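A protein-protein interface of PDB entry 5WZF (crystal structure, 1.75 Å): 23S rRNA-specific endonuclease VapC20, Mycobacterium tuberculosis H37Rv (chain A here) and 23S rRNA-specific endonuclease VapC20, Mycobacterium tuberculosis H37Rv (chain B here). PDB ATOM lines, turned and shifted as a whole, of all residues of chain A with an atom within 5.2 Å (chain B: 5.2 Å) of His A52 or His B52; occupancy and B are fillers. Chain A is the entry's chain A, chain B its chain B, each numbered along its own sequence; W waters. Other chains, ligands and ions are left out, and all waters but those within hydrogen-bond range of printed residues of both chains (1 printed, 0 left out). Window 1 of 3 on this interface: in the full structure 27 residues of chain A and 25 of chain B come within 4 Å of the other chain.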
ATOM      1  N   THR A  19      27.458   1.390  -5.078  1.00  0.00           N
ATOM      2  CA  THR A  19      28.396   1.538  -3.969  1.00  0.00           C
ATOM      3  C   THR A  19      29.848   1.617  -4.426  1.00  0.00           C
ATOM      4  O   THR A  19      30.611   2.460  -3.954  1.00  0.00           O
ATOM      5  CB  THR A  19      28.266   0.360  -2.988  1.00  0.00           C
ATOM      6  OG1 THR A  19      26.901   0.228  -2.578  1.00  0.00           O
ATOM      7  CG2 THR A  19      29.156   0.564  -1.766  1.00  0.00           C
ATOM      8  N   SER A  50      20.273   4.380  -4.665  1.00  0.00           N
ATOM      9  CA  SER A  50      19.258   3.844  -3.759  1.00  0.00           C
ATOM     10  C   SER A  50      19.649   4.017  -2.299  1.00  0.00           C
ATOM     11  O   SER A  50      20.809   4.291  -1.987  1.00  0.00           O
ATOM     12  CB  SER A  50      19.014   2.360  -4.038  1.00  0.00           C
ATOM     13  OG  SER A  50      20.072   1.584  -3.497  1.00  0.00           O
ATOM     14  N   ASN A  51      18.678   3.837  -1.409  1.00  0.00           N
ATOM     15  CA  ASN A  51      18.943   3.893   0.021  1.00  0.00           C
ATOM     16  C   ASN A  51      19.879   2.767   0.450  1.00  0.00           C
ATOM     17  O   ASN A  51      20.775   2.973   1.270  1.00  0.00           O
ATOM     18  CB  ASN A  51      17.632   3.844   0.823  1.00  0.00           C
ATOM     19  CG  ASN A  51      16.796   2.603   0.530  1.00  0.00           C
ATOM     20  OD1 ASN A  51      16.712   2.140  -0.609  1.00  0.00           O
ATOM     21  ND2 ASN A  51      16.163   2.065   1.568  1.00  0.00           N
ATOM     22  N   HIS A  52      19.679   1.581  -0.118  1.00  0.00           N
ATOM     23  CA  HIS A  52      20.537   0.438   0.178  1.00  0.00           C
ATOM     24  C   HIS A  52      21.984   0.695  -0.248  1.00  0.00           C
ATOM     25  O   HIS A  52      22.920   0.350   0.472  1.00  0.00           O
ATOM     26  CB  HIS A  52      20.001  -0.828  -0.501  1.00  0.00           C
ATOM     27  CG  HIS A  52      18.768  -1.382   0.143  1.00  0.00           C
ATOM     28  ND1 HIS A  52      18.812  -2.182   1.264  1.00  0.00           N
ATOM     29  CD2 HIS A  52      17.458  -1.250  -0.173  1.00  0.00           C
ATOM     30  CE1 HIS A  52      17.582  -2.521   1.609  1.00  0.00           C
ATOM     31  NE2 HIS A  52      16.742  -1.970   0.752  1.00  0.00           N
ATOM     32  N   VAL A  53      22.167   1.308  -1.412  1.00  0.00           N
ATOM     33  CA  VAL A  53      23.508   1.628  -1.893  1.00  0.00           C
ATOM     34  C   VAL A  53      24.184   2.655  -0.986  1.00  0.00           C
ATOM     35  O   VAL A  53      25.350   2.493  -0.609  1.00  0.00           O
ATOM     36  CB  VAL A  53      23.477   2.150  -3.353  1.00  0.00           C
ATOM     37  CG1 VAL A  53      24.757   2.903  -3.693  1.00  0.00           C
ATOM     38  CG2 VAL A  53      23.267   0.996  -4.321  1.00  0.00           C
ATOM     39  N   LEU A  54      23.453   3.703  -0.619  1.00  0.00           N
ATOM     40  CA  LEU A  54      24.042   4.744   0.218  1.00  0.00           C
ATOM     41  C   LEU A  54      24.433   4.171   1.573  1.00  0.00           C
ATOM     42  O   LEU A  54      25.496   4.485   2.103  1.00  0.00           O
ATOM     43  CB  LEU A  54      23.084   5.924   0.388  1.00  0.00           C
ATOM     44  CG  LEU A  54      23.018   6.855  -0.827  1.00  0.00           C
ATOM     45  CD1 LEU A  54      22.221   8.114  -0.494  1.00  0.00           C
ATOM     46  CD2 LEU A  54      24.421   7.199  -1.315  1.00  0.00           C
ATOM     47  N   GLY A  55      23.582   3.306   2.112  1.00  0.00           N
ATOM     48  CA  GLY A  55      23.863   2.667   3.384  1.00  0.00           C
ATOM     49  C   GLY A  55      25.121   1.823   3.325  1.00  0.00           C
ATOM     50  O   GLY A  55      25.948   1.853   4.234  1.00  0.00           O
ATOM     51  N   GLU A  56      25.267   1.067   2.243  1.00  0.00           N
ATOM     52  CA  GLU A  56      26.445   0.237   2.055  1.00  0.00           C
ATOM     53  C   GLU A  56      27.675   1.126   1.909  1.00  0.00           C
ATOM     54  O   GLU A  56      28.744   0.822   2.438  1.00  0.00           O
ATOM     55  CB  GLU A  56      26.276  -0.662   0.830  1.00  0.00           C
ATOM     56  CG  GLU A  56      27.346  -1.732   0.670  1.00  0.00           C
ATOM     57  CD  GLU A  56      27.191  -2.521  -0.617  1.00  0.00           C
ATOM     58  OE1 GLU A  56      26.582  -1.999  -1.576  1.00  0.00           O
ATOM     59  OE2 GLU A  56      27.674  -3.672  -0.671  1.00  0.00           O
ATOM     60  N   THR A  57      27.507   2.235   1.197  1.00  0.00           N
ATOM     61  CA  THR A  57      28.593   3.180   0.978  1.00  0.00           C
ATOM     62  C   THR A  57      29.062   3.787   2.296  1.00  0.00           C
ATOM     63  O   THR A  57      30.270   3.879   2.545  1.00  0.00           O
ATOM     64  CB  THR A  57      28.164   4.292   0.010  1.00  0.00           C
ATOM     65  OG1 THR A  57      27.805   3.700  -1.245  1.00  0.00           O
ATOM     66  CG2 THR A  57      29.297   5.288  -0.205  1.00  0.00           C
ATOM     67  N   VAL A  87      14.057   1.806  -1.885  1.00  0.00           N
ATOM     68  CA  VAL A  87      13.624   0.525  -2.423  1.00  0.00           C
ATOM     69  C   VAL A  87      12.402   0.028  -1.662  1.00  0.00           C
ATOM     70  O   VAL A  87      12.448  -0.164  -0.446  1.00  0.00           O
ATOM     71  CB  VAL A  87      14.745  -0.526  -2.360  1.00  0.00           C
ATOM     72  CG1 VAL A  87      14.272  -1.842  -2.956  1.00  0.00           C
ATOM     73  CG2 VAL A  87      15.987  -0.016  -3.092  1.00  0.00           C
ATOM     74  N   GLU A  92      12.068  -5.211  -3.228  1.00  0.00           N
ATOM     75  CA  GLU A  92      12.889  -6.145  -2.468  1.00  0.00           C
ATOM     76  C   GLU A  92      12.424  -7.582  -2.707  1.00  0.00           C
ATOM     77  O   GLU A  92      13.240  -8.490  -2.838  1.00  0.00           O
ATOM     78  CB  GLU A  92      12.863  -5.810  -0.971  1.00  0.00           C
ATOM     79  CG  GLU A  92      13.666  -4.558  -0.613  1.00  0.00           C
ATOM     80  CD  GLU A  92      13.700  -4.279   0.884  1.00  0.00           C
ATOM     81  OE1 GLU A  92      13.012  -4.991   1.636  1.00  0.00           O
ATOM     82  OE2 GLU A  92      14.416  -3.349   1.299  1.00  0.00           O
ATOM     83  N   PHE A 109      22.782  -8.869  -1.869  1.00  0.00           N
ATOM     84  CA  PHE A 109      21.414  -8.374  -1.776  1.00  0.00           C
ATOM     85  C   PHE A 109      21.291  -6.936  -2.287  1.00  0.00           C
ATOM     86  O   PHE A 109      20.344  -6.607  -3.003  1.00  0.00           O
ATOM     87  CB  PHE A 109      20.906  -8.460  -0.334  1.00  0.00           C
ATOM     88  CG  PHE A 109      19.556  -7.834  -0.132  1.00  0.00           C
ATOM     89  CD1 PHE A 109      18.406  -8.507  -0.502  1.00  0.00           C
ATOM     90  CD2 PHE A 109      19.439  -6.572   0.426  1.00  0.00           C
ATOM     91  CE1 PHE A 109      17.164  -7.933  -0.323  1.00  0.00           C
ATOM     92  CE2 PHE A 109      18.200  -5.994   0.610  1.00  0.00           C
ATOM     93  CZ  PHE A 109      17.060  -6.676   0.237  1.00  0.00           C
ATOM     94  N   VAL A 110      22.236  -6.075  -1.920  1.00  0.00           N
ATOM     95  CA  VAL A 110      22.178  -4.687  -2.377  1.00  0.00           C
ATOM     96  C   VAL A 110      22.209  -4.628  -3.905  1.00  0.00           C
ATOM     97  O   VAL A 110      21.425  -3.904  -4.525  1.00  0.00           O
ATOM     98  CB  VAL A 110      23.324  -3.840  -1.792  1.00  0.00           C
ATOM     99  CG1 VAL A 110      23.326  -2.444  -2.413  1.00  0.00           C
ATOM    100  CG2 VAL A 110      23.181  -3.748  -0.281  1.00  0.00           C
ATOM    101  N   THR A 113      18.813  -5.582  -5.362  1.00  0.00           N
ATOM    102  CA  THR A 113      17.842  -4.495  -5.267  1.00  0.00           C
ATOM    103  C   THR A 113      18.173  -3.412  -6.286  1.00  0.00           C
ATOM    104  O   THR A 113      17.275  -2.797  -6.863  1.00  0.00           O
ATOM    105  CB  THR A 113      17.793  -3.871  -3.853  1.00  0.00           C
ATOM    106  OG1 THR A 113      19.065  -3.296  -3.525  1.00  0.00           O
ATOM    107  CG2 THR A 113      17.429  -4.923  -2.817  1.00  0.00           C
ATOM    108  N   THR B  19      22.129  -9.698  12.090  1.00  0.00           N
ATOM    109  CA  THR B  19      22.895 -10.484  11.130  1.00  0.00           C
ATOM    110  C   THR B  19      23.894 -11.440  11.773  1.00  0.00           C
ATOM    111  O   THR B  19      24.040 -12.582  11.335  1.00  0.00           O
ATOM    112  CB  THR B  19      23.656  -9.550  10.179  1.00  0.00           C
ATOM    113  OG1 THR B  19      22.729  -8.630   9.595  1.00  0.00           O
ATOM    114  CG2 THR B  19      24.381 -10.331   9.083  1.00  0.00           C
ATOM    115  N   SER B  50      14.841  -7.176  10.535  1.00  0.00           N
ATOM    116  CA  SER B  50      14.556  -6.136   9.547  1.00  0.00           C
ATOM    117  C   SER B  50      14.947  -6.551   8.137  1.00  0.00           C
ATOM    118  O   SER B  50      15.698  -7.506   7.945  1.00  0.00           O
ATOM    119  CB  SER B  50      15.274  -4.834   9.905  1.00  0.00           C
ATOM    120  OG  SER B  50      16.643  -4.890   9.537  1.00  0.00           O
ATOM    121  N   ASN B  51      14.444  -5.813   7.151  1.00  0.00           N
ATOM    122  CA  ASN B  51      14.794  -6.070   5.760  1.00  0.00           C
ATOM    123  C   ASN B  51      16.288  -5.858   5.528  1.00  0.00           C
ATOM    124  O   ASN B  51      16.921  -6.623   4.804  1.00  0.00           O
ATOM    125  CB  ASN B  51      13.966  -5.186   4.820  1.00  0.00           C
ATOM    126  CG  ASN B  51      14.124  -3.704   5.110  1.00  0.00           C
ATOM    127  OD1 ASN B  51      14.192  -3.287   6.265  1.00  0.00           O
ATOM    128  ND2 ASN B  51      14.187  -2.900   4.053  1.00  0.00           N
ATOM    129  N   HIS B  52      16.861  -4.837   6.166  1.00  0.00           N
ATOM    130  CA  HIS B  52      18.286  -4.573   6.004  1.00  0.00           C
ATOM    131  C   HIS B  52      19.124  -5.712   6.579  1.00  0.00           C
ATOM    132  O   HIS B  52      20.131  -6.110   5.989  1.00  0.00           O
ATOM    133  CB  HIS B  52      18.676  -3.244   6.661  1.00  0.00           C
ATOM    134  CG  HIS B  52      18.192  -2.038   5.918  1.00  0.00           C
ATOM    135  ND1 HIS B  52      18.750  -1.623   4.727  1.00  0.00           N
ATOM    136  CD2 HIS B  52      17.208  -1.150   6.199  1.00  0.00           C
ATOM    137  CE1 HIS B  52      18.128  -0.536   4.306  1.00  0.00           C
ATOM    138  NE2 HIS B  52      17.187  -0.230   5.180  1.00  0.00           N
ATOM    139  N   VAL B  53      18.696  -6.247   7.719  1.00  0.00           N
ATOM    140  CA  VAL B  53      19.408  -7.350   8.356  1.00  0.00           C
ATOM    141  C   VAL B  53      19.341  -8.613   7.498  1.00  0.00           C
ATOM    142  O   VAL B  53      20.357  -9.280   7.286  1.00  0.00           O
ATOM    143  CB  VAL B  53      18.851  -7.652   9.762  1.00  0.00           C
ATOM    144  CG1 VAL B  53      19.275  -9.045  10.223  1.00  0.00           C
ATOM    145  CG2 VAL B  53      19.319  -6.593  10.753  1.00  0.00           C
ATOM    146  N   LEU B  54      18.150  -8.936   7.000  1.00  0.00           N
ATOM    147  CA  LEU B  54      17.993 -10.131   6.177  1.00  0.00           C
ATOM    148  C   LEU B  54      18.850 -10.015   4.925  1.00  0.00           C
ATOM    149  O   LEU B  54      19.479 -10.982   4.500  1.00  0.00           O
ATOM    150  CB  LEU B  54      16.528 -10.360   5.802  1.00  0.00           C
ATOM    151  CG  LEU B  54      15.633 -10.924   6.908  1.00  0.00           C
ATOM    152  CD1 LEU B  54      14.254 -11.296   6.364  1.00  0.00           C
ATOM    153  CD2 LEU B  54      16.301 -12.126   7.572  1.00  0.00           C
ATOM    154  N   GLY B  55      18.878  -8.822   4.343  1.00  0.00           N
ATOM    155  CA  GLY B  55      19.711  -8.576   3.183  1.00  0.00           C
ATOM    156  C   GLY B  55      21.181  -8.791   3.486  1.00  0.00           C
ATOM    157  O   GLY B  55      21.893  -9.430   2.715  1.00  0.00           O
ATOM    158  N   GLU B  56      21.632  -8.262   4.619  1.00  0.00           N
ATOM    159  CA  GLU B  56      23.030  -8.362   5.005  1.00  0.00           C
ATOM    160  C   GLU B  56      23.369  -9.816   5.307  1.00  0.00           C
ATOM    161  O   GLU B  56      24.478 -10.277   5.041  1.00  0.00           O
ATOM    162  CB  GLU B  56      23.318  -7.472   6.219  1.00  0.00           C
ATOM    163  CG  GLU B  56      24.781  -7.393   6.621  1.00  0.00           C
ATOM    164  CD  GLU B  56      24.987  -6.615   7.913  1.00  0.00           C
ATOM    165  OE1 GLU B  56      24.073  -6.612   8.759  1.00  0.00           O
ATOM    166  OE2 GLU B  56      26.060  -6.005   8.075  1.00  0.00           O
ATOM    167  N   THR B  57      22.388 -10.531   5.848  1.00  0.00           N
ATOM    168  CA  THR B  57      22.529 -11.952   6.157  1.00  0.00           C
ATOM    169  C   THR B  57      22.664 -12.799   4.893  1.00  0.00           C
ATOM    170  O   THR B  57      23.511 -13.691   4.835  1.00  0.00           O
ATOM    171  CB  THR B  57      21.337 -12.452   6.990  1.00  0.00           C
ATOM    172  OG1 THR B  57      21.324 -11.756   8.245  1.00  0.00           O
ATOM    173  CG2 THR B  57      21.436 -13.957   7.238  1.00  0.00           C
ATOM    174  N   VAL B  87      12.172  -1.212   7.162  1.00  0.00           N
ATOM    175  CA  VAL B  87      12.536   0.092   7.705  1.00  0.00           C
ATOM    176  C   VAL B  87      12.005   1.208   6.811  1.00  0.00           C
ATOM    177  O   VAL B  87      12.342   1.284   5.631  1.00  0.00           O
ATOM    178  CB  VAL B  87      14.058   0.230   7.862  1.00  0.00           C
ATOM    179  CG1 VAL B  87      14.398   1.564   8.508  1.00  0.00           C
ATOM    180  CG2 VAL B  87      14.609  -0.923   8.695  1.00  0.00           C
ATOM    181  N   GLU B  92      14.793   5.437   8.522  1.00  0.00           N
ATOM    182  CA  GLU B  92      16.113   5.531   7.905  1.00  0.00           C
ATOM    183  C   GLU B  92      16.727   6.917   8.098  1.00  0.00           C
ATOM    184  O   GLU B  92      17.925   7.040   8.340  1.00  0.00           O
ATOM    185  CB  GLU B  92      16.044   5.196   6.411  1.00  0.00           C
ATOM    186  CG  GLU B  92      15.986   3.710   6.125  1.00  0.00           C
ATOM    187  CD  GLU B  92      16.300   3.374   4.677  1.00  0.00           C
ATOM    188  OE1 GLU B  92      16.486   4.308   3.873  1.00  0.00           O
ATOM    189  OE2 GLU B  92      16.371   2.174   4.355  1.00  0.00           O
ATOM    190  N   PHE B 109      25.655   1.170   8.815  1.00  0.00           N
ATOM    191  CA  PHE B 109      24.308   1.629   8.498  1.00  0.00           C
ATOM    192  C   PHE B 109      23.237   0.641   8.962  1.00  0.00           C
ATOM    193  O   PHE B 109      22.215   1.043   9.514  1.00  0.00           O
ATOM    194  CB  PHE B 109      24.164   1.864   6.999  1.00  0.00           C
ATOM    195  CG  PHE B 109      22.759   2.175   6.570  1.00  0.00           C
ATOM    196  CD1 PHE B 109      22.225   3.436   6.768  1.00  0.00           C
ATOM    197  CD2 PHE B 109      21.972   1.204   5.972  1.00  0.00           C
ATOM    198  CE1 PHE B 109      20.932   3.725   6.376  1.00  0.00           C
ATOM    199  CE2 PHE B 109      20.681   1.488   5.576  1.00  0.00           C
ATOM    200  CZ  PHE B 109      20.161   2.750   5.777  1.00  0.00           C
ATOM    201  N   VAL B 110      23.461  -0.649   8.723  1.00  0.00           N
ATOM    202  CA  VAL B 110      22.483  -1.659   9.122  1.00  0.00           C
ATOM    203  C   VAL B 110      22.278  -1.646  10.638  1.00  0.00           C
ATOM    204  O   VAL B 110      21.149  -1.743  11.124  1.00  0.00           O
ATOM    205  CB  VAL B 110      22.903  -3.070   8.651  1.00  0.00           C
ATOM    206  CG1 VAL B 110      22.010  -4.130   9.266  1.00  0.00           C
ATOM    207  CG2 VAL B 110      22.848  -3.154   7.132  1.00  0.00           C
ATOM    208  N   THR B 113      20.091   1.301  11.633  1.00  0.00           N
ATOM    209  CA  THR B 113      18.675   1.084  11.351  1.00  0.00           C
ATOM    210  C   THR B 113      18.098   0.069  12.337  1.00  0.00           C
ATOM    211  O   THR B 113      16.928   0.144  12.704  1.00  0.00           O
ATOM    212  CB  THR B 113      18.433   0.605   9.900  1.00  0.00           C
ATOM    213  OG1 THR B 113      19.109  -0.637   9.672  1.00  0.00           O
ATOM    214  CG2 THR B 113      18.921   1.648   8.899  1.00  0.00           C
HETATM  215  O   HOH W   1      20.624  -2.586   3.137  1.00  0.00           O
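Of chain B, only His B52 (3.4 Å) comes within 4 Å of His A52. Of the printed residues of chain A, Gly B55 touches Phe A109. Printed residues of chain B within 4 Å of Glu A92: Asn B51. Printed residues of chain A within 4 Å of Glu B92: Asn A51 (2.8 Å). The nearest residue of chain B that does not touch His A52 is Asn B51 (4.2 Å).
Among the printed residues, no Asp or Glu carboxylate lies within 4 Å of a Lys or Arg side-chain nitrogen of the other chain.
OE2 of Glu B92 sits at hydrogen-bond distance from ND2 of Asn A51, at 2.8 Å. ND2 of Asn B51 sits at hydrogen-bond distance from OE2 of Glu A92, at 2.8 Å.
His A52 touches His B52. O of Gly A55 touches CB of Phe B109, at 3.3 Å. CB of Phe A109 touches O of Gly B55, 3.3 Å away.
Water W1 bridges a ring nitrogen (ND1) of His A52 (2.6 Å) and a ring nitrogen (ND1) of His B52 (2.6 Å).
OG of Ser A50 lies close to N of His A52 (3.4 Å). The side-chain amide oxygen (OD1) of Asn A51 lies within hydrogen-bond range of the backbone NH (N) of Val A87 (3.0 Å). NE2 of His A52 sits at hydrogen-bond distance from OE2 of Glu A92. OG of Ser B50 lies close to N of His B52 (3.4 Å). The side-chain amide oxygen of Asn B51 sits at hydrogen-bond distance from the backbone NH of Val B87 (3.0 Å). OE2 of Glu B92 lies within hydrogen-bond range of NE2 of His B52, at 2.7 Å.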
